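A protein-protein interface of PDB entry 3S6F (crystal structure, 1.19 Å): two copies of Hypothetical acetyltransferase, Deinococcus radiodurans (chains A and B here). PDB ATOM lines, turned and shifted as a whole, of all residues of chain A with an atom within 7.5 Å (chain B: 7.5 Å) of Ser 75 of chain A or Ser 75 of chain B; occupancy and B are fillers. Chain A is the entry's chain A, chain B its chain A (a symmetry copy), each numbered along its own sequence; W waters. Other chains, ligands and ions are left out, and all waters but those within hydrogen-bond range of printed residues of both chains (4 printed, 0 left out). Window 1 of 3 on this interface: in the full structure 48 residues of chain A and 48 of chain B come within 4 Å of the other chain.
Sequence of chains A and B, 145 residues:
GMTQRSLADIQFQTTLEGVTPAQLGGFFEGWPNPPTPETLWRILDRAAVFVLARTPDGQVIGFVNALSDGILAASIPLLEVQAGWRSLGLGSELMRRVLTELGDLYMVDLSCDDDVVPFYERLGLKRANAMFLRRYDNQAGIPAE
Ala 73 of chain A touches Pro 77 of chain B, and with the chains exchanged Pro 77 of chain A touches Ala 73 of chain B.
Ser 75 of chain A touches its own counterpart, Ser 75 of chain B.
Positions printed for both chains: 48, 49, 65, 66, 67, 68, 69, 73, 74, 75, 76, 77, 78, 98, 102, 105, 107, 108, 109, 110 and 111.
Of the 14 pairs that touch across the chains among the printed residues, 14 have their exchanged pair printed and touching as well.
Of the 21 printed residues of chain B, 9 touch a printed residue of chain A.
Hydrophobic or aromatic side chains of chain B that line the printed part of chain A: Leu 67, Ala 73, Pro 77 and Met 107.
Hydrophobic or aromatic side chains of chain A within 4 Å of the printed part of chain B: Leu 67, Ala 73, Pro 77 and Met 107.
Along chain A the printed residues that touch a printed residue of chain B span positions 67 to 111.
Among the printed residues, no Asp or Glu carboxylate lies within 4 Å of a Lys or Arg side-chain nitrogen of the other chain.
Of the printed residues of chain B, Ser 75 of chain A touches Ser 75.
Of the printed residues of chain A, Ser 75 of chain B touches Ser 75 (2.8 Å).
Printed residues of chain A within 4 Å of Asp 69 of chain B: Leu 67 (3.9 Å).
Printed residues of chain A within 4 Å of Ala 73 of chain B: Leu 67 and Pro 77.
Printed residues of chain A within 4 Å of Pro 77 of chain B: Ala 73 and Met 107.
The nearest printed residue of chain B that does not touch Ser 75 of chain A is Leu 67 of chain B (4.1 Å).
The nearest printed residue of chain A that does not touch Ser 75 of chain B is Leu 67 of chain A (4.1 Å).
The nearest printed residue of chain A that does not touch Ala 73 of chain B is Asn 65 of chain A (5.9 Å).
CB of Leu 67 of chain A touches CB of Leu 67 of chain B, 3.7 Å away.
Asp 69 of chain B touches Leu 67 of chain A.
N of Asp 69 of chain A touches CD2 of Leu 67 of chain B (3.9 Å).
CD1 of Leu 67 of chain B touches O of Ala 73 of chain A, 3.6 Å away.
Ala 73 of chain A touches Pro 77 of chain B (CB to CB, 3.6 Å).
Leu 67 of chain B touches Ala 74 of chain A.
Pro 77 of chain A touches Ala 73 of chain B (CB to CB, 3.6 Å).
O of Pro 77 of chain A touches CE of Met 107 of chain B (3.4 Å).
Pro 77 of chain B touches Met 107 of chain A (O to CE, 3.4 Å).
OG of Ser 75 of chain A lies within hydrogen-bond range of OG of Ser 75 of chain B, 2.8 Å away.
The side-chain carboxylate (OD2) of Asp 109 of chain A is in hydrogen-bond range of the side-chain hydroxyl (OG) of Ser 111 of chain B (2.6 Å).
The side-chain hydroxyl (OG) of Ser 111 of chain A lies within hydrogen-bond range of the side-chain carboxylate (OD2) of Asp 109 of chain B, 2.6 Å away.
N of Ala 74 of chain A sits at hydrogen-bond distance from O of Met 107 of chain A.
The backbone NH (N) of Leu 67 of chain A sits at hydrogen-bond distance from the backbone carbonyl oxygen (O) of Ser 75 of chain A, 2.8 Å away.
The backbone carbonyl oxygen of Asp 109 of chain A sits at hydrogen-bond distance from the backbone NH of Ile 76 of chain A (3.1 Å).
The backbone NH (N) of Ala 74 of chain B lies within hydrogen-bond range of the backbone carbonyl oxygen (O) of Met 107 of chain B, 2.9 Å away.
Water W1 lies within hydrogen-bond range of OD2 of Asp 69 of chain A (2.8 Å) and ND2 of Asn 65 of chain B (3.0 Å).
Water W4 lies within hydrogen-bond range of OD2 of Asp 69 of chain B (2.8 Å) and ND2 of Asn 65 of chain A (3.0 Å).
Water W2 lies within hydrogen-bond range of OD2 of Asp 69 of chain A (2.8 Å) and ND2 of Asn 65 of chain B (2.9 Å).
Water W3 lies within hydrogen-bond range of OD2 of Asp 69 of chain B (2.8 Å) and ND2 of Asn 65 of chain A (2.9 Å).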
ATOM      1  N   ALA A  48       8.158 -22.171  24.584  1.00  0.00           N
ATOM      2  CA  ALA A  48       8.312 -22.659  25.965  1.00  0.00           C
ATOM      3  C   ALA A  48       7.179 -22.159  26.836  1.00  0.00           C
ATOM      4  O   ALA A  48       6.540 -22.925  27.565  1.00  0.00           O
ATOM      5  CB  ALA A  48       9.661 -22.272  26.554  1.00  0.00           C
ATOM      6  N   VAL A  49       6.941 -20.851  26.808  1.00  0.00           N
ATOM      7  CA  VAL A  49       5.879 -20.188  27.554  1.00  0.00           C
ATOM      8  C   VAL A  49       5.384 -19.032  26.707  1.00  0.00           C
ATOM      9  O   VAL A  49       6.076 -18.535  25.796  1.00  0.00           O
ATOM     10  CB  VAL A  49       6.328 -19.688  28.959  1.00  0.00           C
ATOM     11  CG1 VAL A  49       6.772 -20.842  29.878  1.00  0.00           C
ATOM     12  CG2 VAL A  49       7.393 -18.600  28.837  1.00  0.00           C
ATOM     13  N   ASN A  65       5.648 -14.319  23.336  1.00  0.00           N
ATOM     14  CA  ASN A  65       6.114 -15.692  23.457  1.00  0.00           C
ATOM     15  C   ASN A  65       7.564 -15.734  23.899  1.00  0.00           C
ATOM     16  O   ASN A  65       8.282 -14.734  23.852  1.00  0.00           O
ATOM     17  CB  ASN A  65       5.911 -16.508  22.165  1.00  0.00           C
ATOM     18  CG  ASN A  65       6.818 -16.067  21.010  1.00  0.00           C
ATOM     19  OD1 ASN A  65       7.170 -14.898  20.908  1.00  0.00           O
ATOM     20  ND2 ASN A  65       7.107 -17.011  20.107  1.00  0.00           N
ATOM     21  N   ALA A  66       8.024 -16.933  24.270  1.00  0.00           N
ATOM     22  CA  ALA A  66       9.397 -17.100  24.708  1.00  0.00           C
ATOM     23  C   ALA A  66       9.866 -18.516  24.397  1.00  0.00           C
ATOM     24  O   ALA A  66       9.112 -19.500  24.533  1.00  0.00           O
ATOM     25  CB  ALA A  66       9.585 -16.790  26.190  1.00  0.00           C
ATOM     26  N   LEU A  67      11.143 -18.593  24.060  1.00  0.00           N
ATOM     27  CA  LEU A  67      11.902 -19.844  23.949  1.00  0.00           C
ATOM     28  C   LEU A  67      12.717 -19.978  25.213  1.00  0.00           C
ATOM     29  O   LEU A  67      13.169 -18.972  25.768  1.00  0.00           O
ATOM     30  CB  LEU A  67      12.846 -19.775  22.743  1.00  0.00           C
ATOM     31  CG  LEU A  67      12.251 -19.217  21.442  1.00  0.00           C
ATOM     32  CD1 LEU A  67      13.346 -19.167  20.364  1.00  0.00           C
ATOM     33  CD2 LEU A  67      10.993 -19.957  20.963  1.00  0.00           C
ATOM     34  N   SER A  68      12.958 -21.198  25.693  1.00  0.00           N
ATOM     35  CA  SER A  68      13.708 -21.375  26.925  1.00  0.00           C
ATOM     36  C   SER A  68      14.259 -22.791  27.020  1.00  0.00           C
ATOM     37  O   SER A  68      13.649 -23.725  26.495  1.00  0.00           O
ATOM     38  CB  SER A  68      12.757 -21.150  28.113  1.00  0.00           C
ATOM     39  OG  SER A  68      13.485 -21.210  29.323  1.00  0.00           O
ATOM     40  N   ASP A  69      15.382 -22.955  27.738  1.00  0.00           N
ATOM     41  CA  ASP A  69      15.840 -24.270  28.147  1.00  0.00           C
ATOM     42  C   ASP A  69      15.500 -24.586  29.609  1.00  0.00           C
ATOM     43  O   ASP A  69      15.807 -25.670  30.058  1.00  0.00           O
ATOM     44  CB  ASP A  69      17.332 -24.482  27.845  1.00  0.00           C
ATOM     45  CG  ASP A  69      18.276 -23.554  28.565  1.00  0.00           C
ATOM     46  OD1 ASP A  69      17.886 -22.969  29.621  1.00  0.00           O
ATOM     47  OD2 ASP A  69      19.412 -23.383  28.038  1.00  0.00           O
ATOM     48  N   ALA A  73      18.844 -20.129  29.925  1.00  0.00           N
ATOM     49  CA  ALA A  73      18.591 -19.124  28.925  1.00  0.00           C
ATOM     50  C   ALA A  73      17.202 -19.149  28.319  1.00  0.00           C
ATOM     51  O   ALA A  73      16.661 -20.208  28.075  1.00  0.00           O
ATOM     52  CB  ALA A  73      19.650 -19.195  27.782  1.00  0.00           C
ATOM     53  N   ALA A  74      16.735 -17.954  27.984  1.00  0.00           N
ATOM     54  CA  ALA A  74      15.493 -17.752  27.305  1.00  0.00           C
ATOM     55  C   ALA A  74      15.618 -16.580  26.345  1.00  0.00           C
ATOM     56  O   ALA A  74      16.450 -15.685  26.507  1.00  0.00           O
ATOM     57  CB  ALA A  74      14.352 -17.517  28.289  1.00  0.00           C
ATOM     58  N   SER A  75      14.779 -16.578  25.313  1.00  0.00           N
ATOM     59  CA  SER A  75      14.664 -15.423  24.445  1.00  0.00           C
ATOM     60  C   SER A  75      13.218 -15.174  24.071  1.00  0.00           C
ATOM     61  O   SER A  75      12.390 -16.079  24.069  1.00  0.00           O
ATOM     62  CB  SER A  75      15.509 -15.574  23.188  1.00  0.00           C
ATOM     63  OG  SER A  75      14.978 -16.608  22.342  1.00  0.00           O
ATOM     64  N   ILE A  76      12.929 -13.922  23.730  1.00  0.00           N
ATOM     65  CA  ILE A  76      11.560 -13.444  23.492  1.00  0.00           C
ATOM     66  C   ILE A  76      11.415 -13.040  22.029  1.00  0.00           C
ATOM     67  O   ILE A  76      11.815 -11.940  21.670  1.00  0.00           O
ATOM     68  CB  ILE A  76      11.193 -12.297  24.441  1.00  0.00           C
ATOM     69  CG1 ILE A  76      11.286 -12.839  25.933  1.00  0.00           C
ATOM     70  CG2 ILE A  76       9.789 -11.753  24.128  1.00  0.00           C
ATOM     71  CD1 ILE A  76      11.168 -11.817  27.037  1.00  0.00           C
ATOM     72  N   PRO A  77      10.912 -13.934  21.162  1.00  0.00           N
ATOM     73  CA  PRO A  77      10.862 -13.585  19.747  1.00  0.00           C
ATOM     74  C   PRO A  77       9.880 -12.496  19.365  1.00  0.00           C
ATOM     75  O   PRO A  77      10.174 -11.688  18.484  1.00  0.00           O
ATOM     76  CB  PRO A  77      10.499 -14.931  19.070  1.00  0.00           C
ATOM     77  CG  PRO A  77      10.956 -15.984  20.041  1.00  0.00           C
ATOM     78  CD  PRO A  77      10.656 -15.371  21.385  1.00  0.00           C
ATOM     79  N   LEU A  78       8.686 -12.549  19.946  1.00  0.00           N
ATOM     80  CA  LEU A  78       7.546 -11.726  19.528  1.00  0.00           C
ATOM     81  C   LEU A  78       6.853 -11.099  20.709  1.00  0.00           C
ATOM     82  O   LEU A  78       6.570 -11.773  21.703  1.00  0.00           O
ATOM     83  CB  LEU A  78       6.529 -12.565  18.751  1.00  0.00           C
ATOM     84  CG  LEU A  78       6.995 -13.303  17.500  1.00  0.00           C
ATOM     85  CD1 LEU A  78       5.909 -14.291  17.054  1.00  0.00           C
ATOM     86  CD2 LEU A  78       7.395 -12.332  16.375  1.00  0.00           C
ATOM     87  N   VAL A  98       5.502 -12.552  31.184  1.00  0.00           N
ATOM     88  CA  VAL A  98       6.282 -13.623  30.552  1.00  0.00           C
ATOM     89  C   VAL A  98       7.578 -13.872  31.334  1.00  0.00           C
ATOM     90  O   VAL A  98       8.022 -15.016  31.451  1.00  0.00           O
ATOM     91  CB  VAL A  98       6.530 -13.378  29.052  1.00  0.00           C
ATOM     92  CG1 VAL A  98       7.663 -12.398  28.756  1.00  0.00           C
ATOM     93  CG2 VAL A  98       6.767 -14.720  28.347  1.00  0.00           C
ATOM     94  N   LEU A 102       8.858 -17.455  32.852  1.00  0.00           N
ATOM     95  CA  LEU A 102      10.182 -17.977  32.568  1.00  0.00           C
ATOM     96  C   LEU A 102      10.959 -18.344  33.812  1.00  0.00           C
ATOM     97  O   LEU A 102      11.813 -19.237  33.771  1.00  0.00           O
ATOM     98  CB  LEU A 102      10.998 -16.969  31.749  1.00  0.00           C
ATOM     99  CG  LEU A 102      10.614 -16.886  30.272  1.00  0.00           C
ATOM    100  CD1 LEU A 102      11.234 -15.670  29.633  1.00  0.00           C
ATOM    101  CD2 LEU A 102      10.967 -18.191  29.548  1.00  0.00           C
ATOM    102  N   LEU A 105      15.935 -17.467  35.416  1.00  0.00           N
ATOM    103  CA  LEU A 105      17.018 -17.877  34.496  1.00  0.00           C
ATOM    104  C   LEU A 105      18.105 -16.876  34.420  1.00  0.00           C
ATOM    105  O   LEU A 105      17.828 -15.664  34.386  1.00  0.00           O
ATOM    106  CB  LEU A 105      16.497 -17.948  33.057  1.00  0.00           C
ATOM    107  CG  LEU A 105      15.401 -18.954  32.811  1.00  0.00           C
ATOM    108  CD1 LEU A 105      14.813 -18.821  31.408  1.00  0.00           C
ATOM    109  CD2 LEU A 105      15.909 -20.402  33.143  1.00  0.00           C
ATOM    110  N   MET A 107      19.932 -15.901  31.797  1.00  0.00           N
ATOM    111  CA  MET A 107      19.880 -15.056  30.601  1.00  0.00           C
ATOM    112  C   MET A 107      18.477 -14.961  30.044  1.00  0.00           C
ATOM    113  O   MET A 107      17.855 -15.981  29.778  1.00  0.00           O
ATOM    114  CB  MET A 107      20.750 -15.649  29.489  1.00  0.00           C
ATOM    115  CG  MET A 107      22.200 -15.760  29.838  1.00  0.00           C
ATOM    116  SD  MET A 107      23.146 -17.024  28.656  1.00  0.00           S
ATOM    117  CE  MET A 107      22.811 -16.180  26.974  1.00  0.00           C
ATOM    118  N   VAL A 108      18.024 -13.736  29.795  1.00  0.00           N
ATOM    119  CA  VAL A 108      16.835 -13.484  28.979  1.00  0.00           C
ATOM    120  C   VAL A 108      17.238 -12.425  27.978  1.00  0.00           C
ATOM    121  O   VAL A 108      17.751 -11.358  28.376  1.00  0.00           O
ATOM    122  CB  VAL A 108      15.631 -12.999  29.775  1.00  0.00           C
ATOM    123  CG1 VAL A 108      14.421 -12.851  28.848  1.00  0.00           C
ATOM    124  CG2 VAL A 108      15.298 -14.005  30.930  1.00  0.00           C
ATOM    125  N   ASP A 109      17.003 -12.686  26.701  1.00  0.00           N
ATOM    126  CA  ASP A 109      17.463 -11.809  25.649  1.00  0.00           C
ATOM    127  C   ASP A 109      16.408 -11.637  24.565  1.00  0.00           C
ATOM    128  O   ASP A 109      15.585 -12.527  24.306  1.00  0.00           O
ATOM    129  CB  ASP A 109      18.745 -12.376  24.982  1.00  0.00           C
ATOM    130  CG  ASP A 109      19.938 -12.474  25.921  1.00  0.00           C
ATOM    131  OD1 ASP A 109      19.896 -13.284  26.887  1.00  0.00           O
ATOM    132  OD2 ASP A 109      20.931 -11.773  25.696  1.00  0.00           O
ATOM    133  N   LEU A 110      16.453 -10.500  23.875  1.00  0.00           N
ATOM    134  CA  LEU A 110      15.594 -10.229  22.726  1.00  0.00           C
ATOM    135  C   LEU A 110      16.279  -9.221  21.827  1.00  0.00           C
ATOM    136  O   LEU A 110      17.201  -8.538  22.247  1.00  0.00           O
ATOM    137  CB  LEU A 110      14.187  -9.761  23.159  1.00  0.00           C
ATOM    138  CG  LEU A 110      14.144  -8.445  23.938  1.00  0.00           C
ATOM    139  CD1 LEU A 110      14.003  -7.220  22.998  1.00  0.00           C
ATOM    140  CD2 LEU A 110      12.992  -8.488  24.941  1.00  0.00           C
ATOM    141  N   SER A 111      15.823  -9.171  20.590  1.00  0.00           N
ATOM    142  CA  SER A 111      16.308  -8.223  19.572  1.00  0.00           C
ATOM    143  C   SER A 111      15.307  -7.124  19.315  1.00  0.00           C
ATOM    144  O   SER A 111      14.094  -7.361  19.306  1.00  0.00           O
ATOM    145  CB  SER A 111      16.605  -8.926  18.251  1.00  0.00           C
ATOM    146  OG  SER A 111      17.561  -9.966  18.443  1.00  0.00           O
ATOM    147  N   ALA B  48      16.906 -26.985  22.000  1.00  0.00           N
ATOM    148  CA  ALA B  48      16.244 -27.516  20.797  1.00  0.00           C
ATOM    149  C   ALA B  48      17.208 -28.356  19.985  1.00  0.00           C
ATOM    150  O   ALA B  48      16.902 -29.485  19.587  1.00  0.00           O
ATOM    151  CB  ALA B  48      15.641 -26.407  19.947  1.00  0.00           C
ATOM    152  N   VAL B  49      18.378 -27.797  19.686  1.00  0.00           N
ATOM    153  CA  VAL B  49      19.442 -28.454  18.941  1.00  0.00           C
ATOM    154  C   VAL B  49      20.761 -27.958  19.500  1.00  0.00           C
ATOM    155  O   VAL B  49      20.850 -26.890  20.138  1.00  0.00           O
ATOM    156  CB  VAL B  49      19.366 -28.205  17.405  1.00  0.00           C
ATOM    157  CG1 VAL B  49      18.070 -28.760  16.784  1.00  0.00           C
ATOM    158  CG2 VAL B  49      19.580 -26.729  17.080  1.00  0.00           C
ATOM    159  N   ASN B  65      24.733 -24.178  21.390  1.00  0.00           N
ATOM    160  CA  ASN B  65      23.361 -24.621  21.585  1.00  0.00           C
ATOM    161  C   ASN B  65      22.382 -23.634  20.978  1.00  0.00           C
ATOM    162  O   ASN B  65      22.730 -22.498  20.653  1.00  0.00           O
ATOM    163  CB  ASN B  65      23.025 -24.887  23.066  1.00  0.00           C
ATOM    164  CG  ASN B  65      22.971 -23.616  23.922  1.00  0.00           C
ATOM    165  OD1 ASN B  65      23.683 -22.655  23.654  1.00  0.00           O
ATOM    166  ND2 ASN B  65      22.181 -23.676  25.001  1.00  0.00           N
ATOM    167  N   ALA B  66      21.116 -24.052  20.889  1.00  0.00           N
ATOM    168  CA  ALA B  66      20.087 -23.195  20.331  1.00  0.00           C
ATOM    169  C   ALA B  66      18.739 -23.543  20.949  1.00  0.00           C
ATOM    170  O   ALA B  66      18.414 -24.721  21.191  1.00  0.00           O
ATOM    171  CB  ALA B  66      20.012 -23.277  18.810  1.00  0.00           C
ATOM    172  N   LEU B  67      17.944 -22.498  21.118  1.00  0.00           N
ATOM    173  CA  LEU B  67      16.520 -22.580  21.462  1.00  0.00           C
ATOM    174  C   LEU B  67      15.746 -22.365  20.183  1.00  0.00           C
ATOM    175  O   LEU B  67      16.178 -21.597  19.319  1.00  0.00           O
ATOM    176  CB  LEU B  67      16.161 -21.477  22.463  1.00  0.00           C
ATOM    177  CG  LEU B  67      17.137 -21.271  23.631  1.00  0.00           C
ATOM    178  CD1 LEU B  67      16.653 -20.096  24.495  1.00  0.00           C
ATOM    179  CD2 LEU B  67      17.393 -22.539  24.460  1.00  0.00           C
ATOM    180  N   SER B  68      14.581 -22.996  20.026  1.00  0.00           N
ATOM    181  CA  SER B  68      13.818 -22.846  18.799  1.00  0.00           C
ATOM    182  C   SER B  68      12.364 -23.241  19.020  1.00  0.00           C
ATOM    183  O   SER B  68      12.080 -24.100  19.857  1.00  0.00           O
ATOM    184  CB  SER B  68      14.413 -23.785  17.735  1.00  0.00           C
ATOM    185  OG  SER B  68      13.757 -23.582  16.500  1.00  0.00           O
ATOM    186  N   ASP B  69      11.452 -22.654  18.228  1.00  0.00           N
ATOM    187  CA  ASP B  69      10.091 -23.148  18.134  1.00  0.00           C
ATOM    188  C   ASP B  69       9.854 -23.991  16.873  1.00  0.00           C
ATOM    189  O   ASP B  69       8.760 -24.484  16.701  1.00  0.00           O
ATOM    190  CB  ASP B  69       9.056 -22.022  18.277  1.00  0.00           C
ATOM    191  CG  ASP B  69       9.105 -20.959  17.210  1.00  0.00           C
ATOM    192  OD1 ASP B  69       9.655 -21.222  16.098  1.00  0.00           O
ATOM    193  OD2 ASP B  69       8.615 -19.833  17.511  1.00  0.00           O
ATOM    194  N   ALA B  73      11.243 -18.957  14.903  1.00  0.00           N
ATOM    195  CA  ALA B  73      12.318 -18.315  15.616  1.00  0.00           C
ATOM    196  C   ALA B  73      13.230 -19.247  16.389  1.00  0.00           C
ATOM    197  O   ALA B  73      12.767 -20.200  16.984  1.00  0.00           O
ATOM    198  CB  ALA B  73      11.770 -17.218  16.580  1.00  0.00           C
ATOM    199  N   ALA B  74      14.492 -18.847  16.446  1.00  0.00           N
ATOM    200  CA  ALA B  74      15.501 -19.516  17.206  1.00  0.00           C
ATOM    201  C   ALA B  74      16.469 -18.497  17.784  1.00  0.00           C
ATOM    202  O   ALA B  74      16.636 -17.388  17.273  1.00  0.00           O
ATOM    203  CB  ALA B  74      16.247 -20.542  16.361  1.00  0.00           C
ATOM    204  N   SER B  75      17.124 -18.869  18.881  1.00  0.00           N
ATOM    205  CA  SER B  75      18.212 -18.071  19.408  1.00  0.00           C
ATOM    206  C   SER B  75      19.340 -18.956  19.894  1.00  0.00           C
ATOM    207  O   SER B  75      19.141 -20.111  20.255  1.00  0.00           O
ATOM    208  CB  SER B  75      17.749 -17.154  20.532  1.00  0.00           C
ATOM    209  OG  SER B  75      17.382 -17.921  21.691  1.00  0.00           O
ATOM    210  N   ILE B  76      20.540 -18.384  19.916  1.00  0.00           N
ATOM    211  CA  ILE B  76      21.782 -19.117  20.199  1.00  0.00           C
ATOM    212  C   ILE B  76      22.384 -18.603  21.501  1.00  0.00           C
ATOM    213  O   ILE B  76      23.047 -17.573  21.489  1.00  0.00           O
ATOM    214  CB  ILE B  76      22.772 -19.015  19.032  1.00  0.00           C
ATOM    215  CG1 ILE B  76      22.089 -19.654  17.746  1.00  0.00           C
ATOM    216  CG2 ILE B  76      24.096 -19.718  19.373  1.00  0.00           C
ATOM    217  CD1 ILE B  76      22.808 -19.472  16.432  1.00  0.00           C
ATOM    218  N   PRO B  77      22.113 -19.263  22.640  1.00  0.00           N
ATOM    219  CA  PRO B  77      22.608 -18.720  23.899  1.00  0.00           C
ATOM    220  C   PRO B  77      24.109 -18.768  24.100  1.00  0.00           C
ATOM    221  O   PRO B  77      24.679 -17.843  24.678  1.00  0.00           O
ATOM    222  CB  PRO B  77      21.872 -19.576  24.960  1.00  0.00           C
ATOM    223  CG  PRO B  77      20.639 -20.078  24.260  1.00  0.00           C
ATOM    224  CD  PRO B  77      21.118 -20.333  22.854  1.00  0.00           C
ATOM    225  N   LEU B  78      24.718 -19.887  23.723  1.00  0.00           N
ATOM    226  CA  LEU B  78      26.113 -20.198  24.051  1.00  0.00           C
ATOM    227  C   LEU B  78      26.865 -20.707  22.850  1.00  0.00           C
ATOM    228  O   LEU B  78      26.377 -21.579  22.125  1.00  0.00           O
ATOM    229  CB  LEU B  78      26.186 -21.253  25.159  1.00  0.00           C
ATOM    230  CG  LEU B  78      25.496 -20.964  26.488  1.00  0.00           C
ATOM    231  CD1 LEU B  78      25.450 -22.246  27.330  1.00  0.00           C
ATOM    232  CD2 LEU B  78      26.162 -19.797  27.240  1.00  0.00           C
ATOM    233  N   VAL B  98      25.133 -25.435  13.453  1.00  0.00           N
ATOM    234  CA  VAL B  98      23.907 -25.259  14.241  1.00  0.00           C
ATOM    235  C   VAL B  98      22.815 -24.601  13.388  1.00  0.00           C
ATOM    236  O   VAL B  98      21.636 -24.931  13.528  1.00  0.00           O
ATOM    237  CB  VAL B  98      24.151 -24.518  15.569  1.00  0.00           C
ATOM    238  CG1 VAL B  98      24.263 -23.001  15.430  1.00  0.00           C
ATOM    239  CG2 VAL B  98      23.055 -24.897  16.575  1.00  0.00           C
ATOM    240  N   LEU B 102      19.032 -26.036  12.745  1.00  0.00           N
ATOM    241  CA  LEU B 102      17.854 -25.220  12.977  1.00  0.00           C
ATOM    242  C   LEU B 102      16.925 -25.160  11.787  1.00  0.00           C
ATOM    243  O   LEU B 102      15.712 -24.986  11.953  1.00  0.00           O
ATOM    244  CB  LEU B 102      18.254 -23.793  13.372  1.00  0.00           C
ATOM    245  CG  LEU B 102      18.753 -23.642  14.808  1.00  0.00           C
ATOM    246  CD1 LEU B 102      19.410 -22.300  15.001  1.00  0.00           C
ATOM    247  CD2 LEU B 102      17.619 -23.905  15.805  1.00  0.00           C
ATOM    248  N   LEU B 105      14.350 -21.223   9.344  1.00  0.00           N
ATOM    249  CA  LEU B 105      13.494 -20.358  10.184  1.00  0.00           C
ATOM    250  C   LEU B 105      13.620 -18.926   9.836  1.00  0.00           C
ATOM    251  O   LEU B 105      14.740 -18.449   9.576  1.00  0.00           O
ATOM    252  CB  LEU B 105      13.952 -20.412  11.645  1.00  0.00           C
ATOM    253  CG  LEU B 105      13.871 -21.767  12.302  1.00  0.00           C
ATOM    254  CD1 LEU B 105      14.525 -21.768  13.682  1.00  0.00           C
ATOM    255  CD2 LEU B 105      12.386 -22.277  12.312  1.00  0.00           C
ATOM    256  N   MET B 107      13.620 -16.236  11.820  1.00  0.00           N
ATOM    257  CA  MET B 107      14.474 -15.475  12.736  1.00  0.00           C
ATOM    258  C   MET B 107      15.482 -16.363  13.432  1.00  0.00           C
ATOM    259  O   MET B 107      15.102 -17.351  14.047  1.00  0.00           O
ATOM    260  CB  MET B 107      13.632 -14.827  13.838  1.00  0.00           C
ATOM    261  CG  MET B 107      12.612 -13.855  13.339  1.00  0.00           C
ATOM    262  SD  MET B 107      11.209 -13.507  14.681  1.00  0.00           S
ATOM    263  CE  MET B 107      12.300 -12.834  16.098  1.00  0.00           C
ATOM    264  N   VAL B 108      16.748 -15.958  13.396  1.00  0.00           N
ATOM    265  CA  VAL B 108      17.782 -16.521  14.267  1.00  0.00           C
ATOM    266  C   VAL B 108      18.497 -15.338  14.876  1.00  0.00           C
ATOM    267  O   VAL B 108      18.962 -14.446  14.135  1.00  0.00           O
ATOM    268  CB  VAL B 108      18.787 -17.404  13.540  1.00  0.00           C
ATOM    269  CG1 VAL B 108      19.768 -18.012  14.547  1.00  0.00           C
ATOM    270  CG2 VAL B 108      18.050 -18.546  12.758  1.00  0.00           C
ATOM    271  N   ASP B 109      18.611 -15.320  16.196  1.00  0.00           N
ATOM    272  CA  ASP B 109      19.157 -14.180  16.896  1.00  0.00           C
ATOM    273  C   ASP B 109      20.083 -14.610  18.025  1.00  0.00           C
ATOM    274  O   ASP B 109      19.927 -15.683  18.627  1.00  0.00           O
ATOM    275  CB  ASP B 109      18.022 -13.318  17.511  1.00  0.00           C
ATOM    276  CG  ASP B 109      17.089 -12.699  16.481  1.00  0.00           C
ATOM    277  OD1 ASP B 109      16.351 -13.451  15.788  1.00  0.00           O
ATOM    278  OD2 ASP B 109      17.059 -11.468  16.370  1.00  0.00           O
ATOM    279  N   LEU B 110      21.036 -13.746  18.366  1.00  0.00           N
ATOM    280  CA  LEU B 110      21.929 -13.951  19.503  1.00  0.00           C
ATOM    281  C   LEU B 110      22.418 -12.603  19.992  1.00  0.00           C
ATOM    282  O   LEU B 110      22.330 -11.614  19.280  1.00  0.00           O
ATOM    283  CB  LEU B 110      23.094 -14.902  19.155  1.00  0.00           C
ATOM    284  CG  LEU B 110      24.041 -14.406  18.060  1.00  0.00           C
ATOM    285  CD1 LEU B 110      25.210 -13.570  18.640  1.00  0.00           C
ATOM    286  CD2 LEU B 110      24.575 -15.602  17.273  1.00  0.00           C
ATOM    287  N   SER B 111      22.903 -12.593  21.218  1.00  0.00           N
ATOM    288  CA  SER B 111      23.485 -11.403  21.863  1.00  0.00           C
ATOM    289  C   SER B 111      24.989 -11.495  21.945  1.00  0.00           C
ATOM    290  O   SER B 111      25.546 -12.571  22.183  1.00  0.00           O
ATOM    291  CB  SER B 111      22.935 -11.207  23.273  1.00  0.00           C
ATOM    292  OG  SER B 111      21.514 -11.101  23.243  1.00  0.00           O
HETATM  293  O   HOH W   1      21.741 -22.018  27.461  1.00  0.00           O
HETATM  294  O   HOH W   2      19.951 -25.210  25.974  1.00  0.00           O
HETATM  295  O   HOH W   3       7.142 -19.880  19.902  1.00  0.00           O
HETATM  296  O   HOH W   4       8.335 -17.091  17.371  1.00  0.00           O
